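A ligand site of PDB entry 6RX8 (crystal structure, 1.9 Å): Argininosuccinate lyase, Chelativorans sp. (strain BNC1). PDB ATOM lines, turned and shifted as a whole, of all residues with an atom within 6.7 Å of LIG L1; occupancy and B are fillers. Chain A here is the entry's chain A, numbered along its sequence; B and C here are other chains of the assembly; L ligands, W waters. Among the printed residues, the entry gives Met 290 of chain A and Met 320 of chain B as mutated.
The backbone NH (N) of Arg 112 of chain B lies within hydrogen-bond range of an oxygen (O3) of LIG L1 (2.9 Å). An oxygen (O1) of LIG L1 sits at hydrogen-bond distance from the side-chain amide nitrogen of Asn 288. The side-chain hydroxyl (OG) of Ser 280 sits close to an oxygen (O4) of LIG L1 (3.5 Å). The side-chain hydroxyl (OG) of Ser 111 of chain B sits at hydrogen-bond distance from an oxygen (O3) of LIG L1. O4 of LIG L1 is in salt-bridge range of NE of Arg 112 of chain B (2.8 Å). The side-chain hydroxyl (OG) of Ser 281 sits at hydrogen-bond distance from an oxygen (O3) of LIG L1 (2.7 Å). N of Ser 281 lies within hydrogen-bond range of O4 of LIG L1, at 2.9 Å. NE of Arg 112 of chain B lies within salt-bridge range of O2 of LG2 L2. OG1 of Thr 158 of chain C sits at hydrogen-bond distance from O2 of LIG L1, at 2.7 Å. The side-chain amino group (NZ) of Lys 286 is in salt-bridge range of an oxygen (O1) of LIG L1. The side-chain amide nitrogen (NE2) of Gln 159 of chain C lies close to an oxygen (O1) of LIG L1 (3.5 Å). ND2 of Asn 113 of chain B lies within hydrogen-bond range of O2 of LIG L1 (2.9 Å).
The side-chain amide oxygen (OD1) of Asn 288 lies within hydrogen-bond range of the side-chain amino group (NZ) of Lys 286. N of Arg 112 of chain B is in hydrogen-bond range of OG of Ser 281 (3.4 Å). OE1 of Gln 159 of chain C sits close to ND2 of Asn 288 (3.3 Å). The backbone NH (N) of Gln 159 of chain C lies within hydrogen-bond range of the backbone carbonyl oxygen (O) of Met 320 of chain B, at 3.0 Å. NH2 of Arg 112 of chain B sits at hydrogen-bond distance from O of Thr 279, 2.9 Å away. O of Ala 202 of chain B is in hydrogen-bond range of ND2 of Asn 113 of chain B (2.9 Å). N of Asn 113 of chain B lies within hydrogen-bond range of OG of Ser 111 of chain B (2.9 Å). The side-chain hydroxyl (OG1) of Thr 158 of chain C sits at hydrogen-bond distance from the side-chain amino group (NZ) of Lys 286, 2.7 Å away.
Merely in contact with LIG L1: Ile 282 and Met 283. Hydrophobic or aromatic side chains within 4 Å of LIG L1: Ile 282 and Met 283. 11 residues have an atom within 4 Å of LIG L1: Ser 280, Ser 281, Ile 282, Met 283, Lys 286, Asn 288, Ser 111 of chain B, Arg 112 of chain B, Asn 113 of chain B, Thr 158 of chain C and Gln 159 of chain C.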
ATOM      1  N   THR A 279     -12.055 -29.003 -12.339  1.00  0.00           N
ATOM      2  CA  THR A 279     -11.932 -27.877 -11.422  1.00  0.00           C
ATOM      3  C   THR A 279     -11.753 -28.436 -10.015  1.00  0.00           C
ATOM      4  O   THR A 279     -11.504 -29.628  -9.830  1.00  0.00           O
ATOM      5  CB  THR A 279     -13.115 -26.908 -11.514  1.00  0.00           C
ATOM      6  OG1 THR A 279     -12.803 -25.718 -10.762  1.00  0.00           O
ATOM      7  CG2 THR A 279     -14.424 -27.558 -10.998  1.00  0.00           C
ATOM      8  N   SER A 280     -11.862 -27.538  -9.043  1.00  0.00           N
ATOM      9  CA  SER A 280     -11.650 -27.860  -7.638  1.00  0.00           C
ATOM     10  C   SER A 280     -12.978 -27.854  -6.881  1.00  0.00           C
ATOM     11  O   SER A 280     -13.850 -27.021  -7.156  1.00  0.00           O
ATOM     12  CB  SER A 280     -10.682 -26.863  -6.990  1.00  0.00           C
ATOM     13  OG  SER A 280     -10.665 -27.025  -5.583  1.00  0.00           O
ATOM     14  N   SER A 281     -13.108 -28.755  -5.920  1.00  0.00           N
ATOM     15  CA  SER A 281     -14.284 -28.738  -5.059  1.00  0.00           C
ATOM     16  C   SER A 281     -14.298 -27.558  -4.104  1.00  0.00           C
ATOM     17  O   SER A 281     -15.339 -27.302  -3.485  1.00  0.00           O
ATOM     18  CB  SER A 281     -14.365 -30.035  -4.253  1.00  0.00           C
ATOM     19  OG  SER A 281     -13.347 -30.090  -3.265  1.00  0.00           O
ATOM     20  N   ILE A 282     -13.171 -26.871  -3.924  1.00  0.00           N
ATOM     21  CA  ILE A 282     -13.045 -25.799  -2.949  1.00  0.00           C
ATOM     22  C   ILE A 282     -12.682 -24.469  -3.599  1.00  0.00           C
ATOM     23  O   ILE A 282     -13.259 -23.439  -3.256  1.00  0.00           O
ATOM     24  CB  ILE A 282     -12.016 -26.178  -1.854  1.00  0.00           C
ATOM     25  CG1 ILE A 282     -11.773 -24.998  -0.911  1.00  0.00           C
ATOM     26  CG2 ILE A 282     -10.721 -26.663  -2.483  1.00  0.00           C
ATOM     27  CD1 ILE A 282     -11.038 -25.393   0.369  1.00  0.00           C
ATOM     28  N   MET A 283     -11.746 -24.478  -4.549  1.00  0.00           N
ATOM     29  CA  MET A 283     -11.196 -23.272  -5.156  1.00  0.00           C
ATOM     30  C   MET A 283     -11.923 -22.991  -6.451  1.00  0.00           C
ATOM     31  O   MET A 283     -11.613 -23.627  -7.473  1.00  0.00           O
ATOM     32  CB  MET A 283      -9.693 -23.430  -5.411  1.00  0.00           C
ATOM     33  CG  MET A 283      -8.860 -23.438  -4.142  1.00  0.00           C
ATOM     34  SD  MET A 283      -7.149 -23.931  -4.344  1.00  0.00           S
ATOM     35  CE  MET A 283      -7.372 -25.634  -4.839  1.00  0.00           C
ATOM     36  N   LYS A 286     -10.144 -22.632 -10.154  1.00  0.00           N
ATOM     37  CA  LYS A 286      -9.277 -23.630 -10.776  1.00  0.00           C
ATOM     38  C   LYS A 286      -9.812 -24.110 -12.119  1.00  0.00           C
ATOM     39  O   LYS A 286     -10.990 -24.470 -12.256  1.00  0.00           O
ATOM     40  CB  LYS A 286      -9.100 -24.846  -9.862  1.00  0.00           C
ATOM     41  CG  LYS A 286      -8.133 -24.651  -8.718  1.00  0.00           C
ATOM     42  CD  LYS A 286      -6.774 -24.161  -9.210  1.00  0.00           C
ATOM     43  CE  LYS A 286      -5.640 -24.673  -8.335  1.00  0.00           C
ATOM     44  NZ  LYS A 286      -5.416 -26.138  -8.547  1.00  0.00           N
ATOM     45  N   ASN A 288      -8.179 -27.021 -13.872  1.00  0.00           N
ATOM     46  CA  ASN A 288      -7.083 -27.924 -13.540  1.00  0.00           C
ATOM     47  C   ASN A 288      -6.716 -28.789 -14.731  1.00  0.00           C
ATOM     48  O   ASN A 288      -7.611 -29.304 -15.414  1.00  0.00           O
ATOM     49  CB  ASN A 288      -7.449 -28.823 -12.375  1.00  0.00           C
ATOM     50  CG  ASN A 288      -7.344 -28.110 -11.047  1.00  0.00           C
ATOM     51  OD1 ASN A 288      -6.533 -27.194 -10.888  1.00  0.00           O
ATOM     52  ND2 ASN A 288      -8.176 -28.513 -10.097  1.00  0.00           N
ATOM     53  N   MET A 290      -6.203 -31.697 -15.398  1.00  0.00           N
ATOM     54  CA  MET A 290      -6.377 -33.040 -14.882  1.00  0.00           C
ATOM     55  C   MET A 290      -6.139 -34.086 -15.950  1.00  0.00           C
ATOM     56  O   MET A 290      -5.619 -35.161 -15.652  1.00  0.00           O
ATOM     57  CB  MET A 290      -7.764 -33.174 -14.269  1.00  0.00           C
ATOM     58  CG  MET A 290      -8.054 -34.509 -13.636  1.00  0.00           C
ATOM     59  SD  MET A 290      -6.917 -34.943 -12.317  1.00  0.00           S
ATOM     60  CE  MET A 290      -7.372 -33.766 -11.052  1.00  0.00           C
ATOM     61  N   LEU B  89     -17.189 -35.790  -5.360  1.00  0.00           N
ATOM     62  CA  LEU B  89     -18.214 -34.885  -5.873  1.00  0.00           C
ATOM     63  C   LEU B  89     -19.495 -35.619  -6.253  1.00  0.00           C
ATOM     64  O   LEU B  89     -20.582 -35.108  -5.944  1.00  0.00           O
ATOM     65  CB  LEU B  89     -17.673 -34.067  -7.042  1.00  0.00           C
ATOM     66  CG  LEU B  89     -16.794 -32.882  -6.595  1.00  0.00           C
ATOM     67  CD1 LEU B  89     -16.351 -32.086  -7.815  1.00  0.00           C
ATOM     68  CD2 LEU B  89     -17.531 -31.944  -5.618  1.00  0.00           C
ATOM     69  N   HIS B 107     -18.613 -29.894   3.457  1.00  0.00           N
ATOM     70  CA  HIS B 107     -17.308 -29.641   2.865  1.00  0.00           C
ATOM     71  C   HIS B 107     -16.671 -28.354   3.361  1.00  0.00           C
ATOM     72  O   HIS B 107     -15.596 -27.965   2.884  1.00  0.00           O
ATOM     73  CB  HIS B 107     -17.421 -29.592   1.349  1.00  0.00           C
ATOM     74  CG  HIS B 107     -16.191 -30.025   0.619  1.00  0.00           C
ATOM     75  ND1 HIS B 107     -15.450 -31.115   0.997  1.00  0.00           N
ATOM     76  CD2 HIS B 107     -15.580 -29.523  -0.483  1.00  0.00           C
ATOM     77  CE1 HIS B 107     -14.434 -31.274   0.162  1.00  0.00           C
ATOM     78  NE2 HIS B 107     -14.503 -30.322  -0.752  1.00  0.00           N
ATOM     79  N   ARG B 110     -12.835 -27.808   3.947  1.00  0.00           N
ATOM     80  CA  ARG B 110     -12.290 -29.080   3.506  1.00  0.00           C
ATOM     81  C   ARG B 110     -12.092 -29.075   2.006  1.00  0.00           C
ATOM     82  O   ARG B 110     -12.685 -28.293   1.262  1.00  0.00           O
ATOM     83  CB  ARG B 110     -13.214 -30.233   3.912  1.00  0.00           C
ATOM     84  CG  ARG B 110     -12.619 -31.617   3.751  1.00  0.00           C
ATOM     85  CD  ARG B 110     -13.595 -32.686   4.255  1.00  0.00           C
ATOM     86  NE  ARG B 110     -14.808 -32.757   3.450  1.00  0.00           N
ATOM     87  CZ  ARG B 110     -15.750 -33.680   3.611  1.00  0.00           C
ATOM     88  NH1 ARG B 110     -15.605 -34.607   4.564  1.00  0.00           N
ATOM     89  NH2 ARG B 110     -16.814 -33.689   2.832  1.00  0.00           N
ATOM     90  N   SER B 111     -11.245 -29.989   1.564  1.00  0.00           N
ATOM     91  CA  SER B 111     -10.909 -30.164   0.164  1.00  0.00           C
ATOM     92  C   SER B 111     -11.023 -31.641  -0.187  1.00  0.00           C
ATOM     93  O   SER B 111     -11.016 -32.509   0.692  1.00  0.00           O
ATOM     94  CB  SER B 111      -9.493 -29.650  -0.117  1.00  0.00           C
ATOM     95  OG  SER B 111      -9.102 -29.874  -1.458  1.00  0.00           O
ATOM     96  N   ARG B 112     -11.089 -31.933  -1.482  1.00  0.00           N
ATOM     97  CA  ARG B 112     -10.790 -33.293  -1.888  1.00  0.00           C
ATOM     98  C   ARG B 112      -9.333 -33.664  -1.599  1.00  0.00           C
ATOM     99  O   ARG B 112      -9.022 -34.857  -1.463  1.00  0.00           O
ATOM    100  CB  ARG B 112     -11.089 -33.485  -3.376  1.00  0.00           C
ATOM    101  CG  ARG B 112     -12.579 -33.592  -3.669  1.00  0.00           C
ATOM    102  CD  ARG B 112     -12.856 -33.911  -5.138  1.00  0.00           C
ATOM    103  NE  ARG B 112     -12.315 -32.883  -6.013  1.00  0.00           N
ATOM    104  CZ  ARG B 112     -12.448 -32.874  -7.342  1.00  0.00           C
ATOM    105  NH1 ARG B 112     -13.126 -33.834  -7.955  1.00  0.00           N
ATOM    106  NH2 ARG B 112     -11.880 -31.907  -8.046  1.00  0.00           N
ATOM    107  N   ASN B 113      -8.445 -32.684  -1.498  1.00  0.00           N
ATOM    108  CA  ASN B 113      -7.031 -33.013  -1.347  1.00  0.00           C
ATOM    109  C   ASN B 113      -6.731 -33.566   0.033  1.00  0.00           C
ATOM    110  O   ASN B 113      -6.075 -34.611   0.159  1.00  0.00           O
ATOM    111  CB  ASN B 113      -6.179 -31.776  -1.626  1.00  0.00           C
ATOM    112  CG  ASN B 113      -6.385 -31.233  -3.022  1.00  0.00           C
ATOM    113  OD1 ASN B 113      -6.985 -31.896  -3.877  1.00  0.00           O
ATOM    114  ND2 ASN B 113      -5.895 -30.030  -3.267  1.00  0.00           N
ATOM    115  N   ASP B 114      -7.195 -32.891   1.095  1.00  0.00           N
ATOM    116  CA  ASP B 114      -6.905 -33.445   2.415  1.00  0.00           C
ATOM    117  C   ASP B 114      -7.823 -34.623   2.714  1.00  0.00           C
ATOM    118  O   ASP B 114      -7.380 -35.593   3.358  1.00  0.00           O
ATOM    119  CB  ASP B 114      -6.927 -32.353   3.493  1.00  0.00           C
ATOM    120  CG  ASP B 114      -8.271 -31.682   3.701  1.00  0.00           C
ATOM    121  OD1 ASP B 114      -9.110 -31.645   2.781  1.00  0.00           O
ATOM    122  OD2 ASP B 114      -8.450 -31.115   4.808  1.00  0.00           O
ATOM    123  N   ALA B 201      -7.054 -28.687   4.116  1.00  0.00           N
ATOM    124  CA  ALA B 201      -7.985 -28.290   3.042  1.00  0.00           C
ATOM    125  C   ALA B 201      -7.258 -28.417   1.718  1.00  0.00           C
ATOM    126  O   ALA B 201      -6.693 -29.478   1.399  1.00  0.00           O
ATOM    127  CB  ALA B 201      -8.546 -26.918   3.337  1.00  0.00           C
ATOM    128  N   ALA B 202      -7.235 -27.378   0.886  1.00  0.00           N
ATOM    129  CA  ALA B 202      -6.675 -27.494  -0.434  1.00  0.00           C
ATOM    130  C   ALA B 202      -5.170 -27.698  -0.370  1.00  0.00           C
ATOM    131  O   ALA B 202      -4.612 -28.411  -1.212  1.00  0.00           O
ATOM    132  CB  ALA B 202      -7.003 -26.253  -1.275  1.00  0.00           C
ATOM    133  N   THR B 203      -4.515 -27.085   0.615  1.00  0.00           N
ATOM    134  CA  THR B 203      -3.056 -27.064   0.727  1.00  0.00           C
ATOM    135  C   THR B 203      -2.578 -25.952   1.647  1.00  0.00           C
ATOM    136  O   THR B 203      -1.385 -25.893   1.978  1.00  0.00           O
ATOM    137  CB  THR B 203      -2.399 -26.871  -0.643  1.00  0.00           C
ATOM    138  OG1 THR B 203      -0.965 -26.870  -0.478  1.00  0.00           O
ATOM    139  CG2 THR B 203      -2.806 -25.555  -1.265  1.00  0.00           C
ATOM    140  N   MET B 320       0.402 -30.724  -3.997  1.00  0.00           N
ATOM    141  CA  MET B 320      -0.630 -31.669  -4.391  1.00  0.00           C
ATOM    142  C   MET B 320      -0.579 -31.817  -5.904  1.00  0.00           C
ATOM    143  O   MET B 320      -0.503 -30.822  -6.628  1.00  0.00           O
ATOM    144  CB  MET B 320      -2.014 -31.202  -3.943  1.00  0.00           C
ATOM    145  CG  MET B 320      -3.160 -32.143  -4.331  1.00  0.00           C
ATOM    146  SD  MET B 320      -3.635 -31.970  -6.078  1.00  0.00           S
ATOM    147  CE  MET B 320      -4.726 -33.375  -6.247  1.00  0.00           C
ATOM    148  N   TYR C 157       0.738 -23.526  -5.078  1.00  0.00           N
ATOM    149  CA  TYR C 157       0.201 -24.199  -6.243  1.00  0.00           C
ATOM    150  C   TYR C 157      -0.316 -25.576  -5.863  1.00  0.00           C
ATOM    151  O   TYR C 157       0.208 -26.250  -4.975  1.00  0.00           O
ATOM    152  CB  TYR C 157       1.264 -24.345  -7.352  1.00  0.00           C
ATOM    153  CG  TYR C 157       1.763 -23.020  -7.846  1.00  0.00           C
ATOM    154  CD1 TYR C 157       2.771 -22.343  -7.172  1.00  0.00           C
ATOM    155  CD2 TYR C 157       1.192 -22.413  -8.959  1.00  0.00           C
ATOM    156  CE1 TYR C 157       3.210 -21.107  -7.595  1.00  0.00           C
ATOM    157  CE2 TYR C 157       1.631 -21.178  -9.391  1.00  0.00           C
ATOM    158  CZ  TYR C 157       2.634 -20.520  -8.705  1.00  0.00           C
ATOM    159  OH  TYR C 157       3.043 -19.285  -9.149  1.00  0.00           O
ATOM    160  N   THR C 158      -1.371 -25.987  -6.555  1.00  0.00           N
ATOM    161  CA  THR C 158      -1.708 -27.395  -6.691  1.00  0.00           C
ATOM    162  C   THR C 158      -1.914 -27.667  -8.175  1.00  0.00           C
ATOM    163  O   THR C 158      -2.516 -26.850  -8.884  1.00  0.00           O
ATOM    164  CB  THR C 158      -2.958 -27.779  -5.887  1.00  0.00           C
ATOM    165  OG1 THR C 158      -4.100 -27.106  -6.431  1.00  0.00           O
ATOM    166  CG2 THR C 158      -2.807 -27.450  -4.414  1.00  0.00           C
ATOM    167  N   GLN C 159      -1.432 -28.813  -8.646  1.00  0.00           N
ATOM    168  CA  GLN C 159      -1.555 -29.169 -10.064  1.00  0.00           C
ATOM    169  C   GLN C 159      -0.968 -28.079 -10.957  1.00  0.00           C
ATOM    170  O   GLN C 159      -1.445 -27.845 -12.075  1.00  0.00           O
ATOM    171  CB  GLN C 159      -3.031 -29.458 -10.412  1.00  0.00           C
ATOM    172  CG  GLN C 159      -3.645 -30.480  -9.439  1.00  0.00           C
ATOM    173  CD  GLN C 159      -5.152 -30.641  -9.574  1.00  0.00           C
ATOM    174  OE1 GLN C 159      -5.675 -30.634 -10.672  1.00  0.00           O
ATOM    175  NE2 GLN C 159      -5.845 -30.776  -8.455  1.00  0.00           N
ATOM    176  N   LYS C 161      -1.182 -24.977 -10.753  1.00  0.00           N
ATOM    177  CA  LYS C 161      -2.102 -23.866 -10.896  1.00  0.00           C
ATOM    178  C   LYS C 161      -2.189 -23.128  -9.568  1.00  0.00           C
ATOM    179  O   LYS C 161      -2.150 -23.752  -8.499  1.00  0.00           O
ATOM    180  CB  LYS C 161      -3.499 -24.344 -11.317  1.00  0.00           C
ATOM    181  CG  LYS C 161      -3.606 -24.686 -12.807  1.00  0.00           C
ATOM    182  CD  LYS C 161      -3.402 -23.424 -13.645  1.00  0.00           C
ATOM    183  CE  LYS C 161      -4.244 -23.461 -14.918  1.00  0.00           C
ATOM    184  NZ  LYS C 161      -4.173 -22.160 -15.614  1.00  0.00           N
ATOM    185  N   ALA C 163      -3.346 -21.749  -6.302  1.00  0.00           N
ATOM    186  CA  ALA C 163      -4.364 -22.316  -5.435  1.00  0.00           C
ATOM    187  C   ALA C 163      -4.846 -21.287  -4.422  1.00  0.00           C
ATOM    188  O   ALA C 163      -5.985 -20.817  -4.513  1.00  0.00           O
ATOM    189  CB  ALA C 163      -3.849 -23.569  -4.718  1.00  0.00           C
HETATM  190  O1  LIG L   1      -7.218 -27.766  -7.465  1.00  0.00           O
HETATM  191  C1  LIG L   1      -7.196 -28.532  -6.477  1.00  0.00           C
HETATM  192  O2  LIG L   1      -6.176 -28.634  -5.745  1.00  0.00           O
HETATM  193  C2  LIG L   1      -8.435 -29.295  -6.206  1.00  0.00           C
HETATM  194  C3  LIG L   1      -9.015 -29.182  -5.017  1.00  0.00           C
HETATM  195  C4  LIG L   1     -10.265 -29.905  -4.671  1.00  0.00           C
HETATM  196  O3  LIG L   1     -10.696 -29.891  -3.494  1.00  0.00           O
HETATM  197  O4  LIG L   1     -10.880 -30.507  -5.576  1.00  0.00           O
HETATM  198  O1  LG2 L   2     -10.088 -35.840  -6.772  1.00  0.00           O
HETATM  199  C1  LG2 L   2      -9.707 -34.785  -7.333  1.00  0.00           C
HETATM  200  O2  LG2 L   2      -9.037 -33.915  -6.758  1.00  0.00           O
HETATM  201  C2  LG2 L   2     -10.025 -34.533  -8.752  1.00  0.00           C
HETATM  202  C3  LG2 L   2     -10.240 -35.536  -9.598  1.00  0.00           C
HETATM  203  C4  LG2 L   2     -10.543 -35.260 -11.010  1.00  0.00           C
HETATM  204  O3  LG2 L   2     -10.342 -36.235 -11.746  1.00  0.00           O
HETATM  205  O4  LG2 L   2     -10.950 -34.145 -11.442  1.00  0.00           O
HETATM  206  O   HOH W   1      -8.603 -31.455  -8.474  1.00  0.00           O
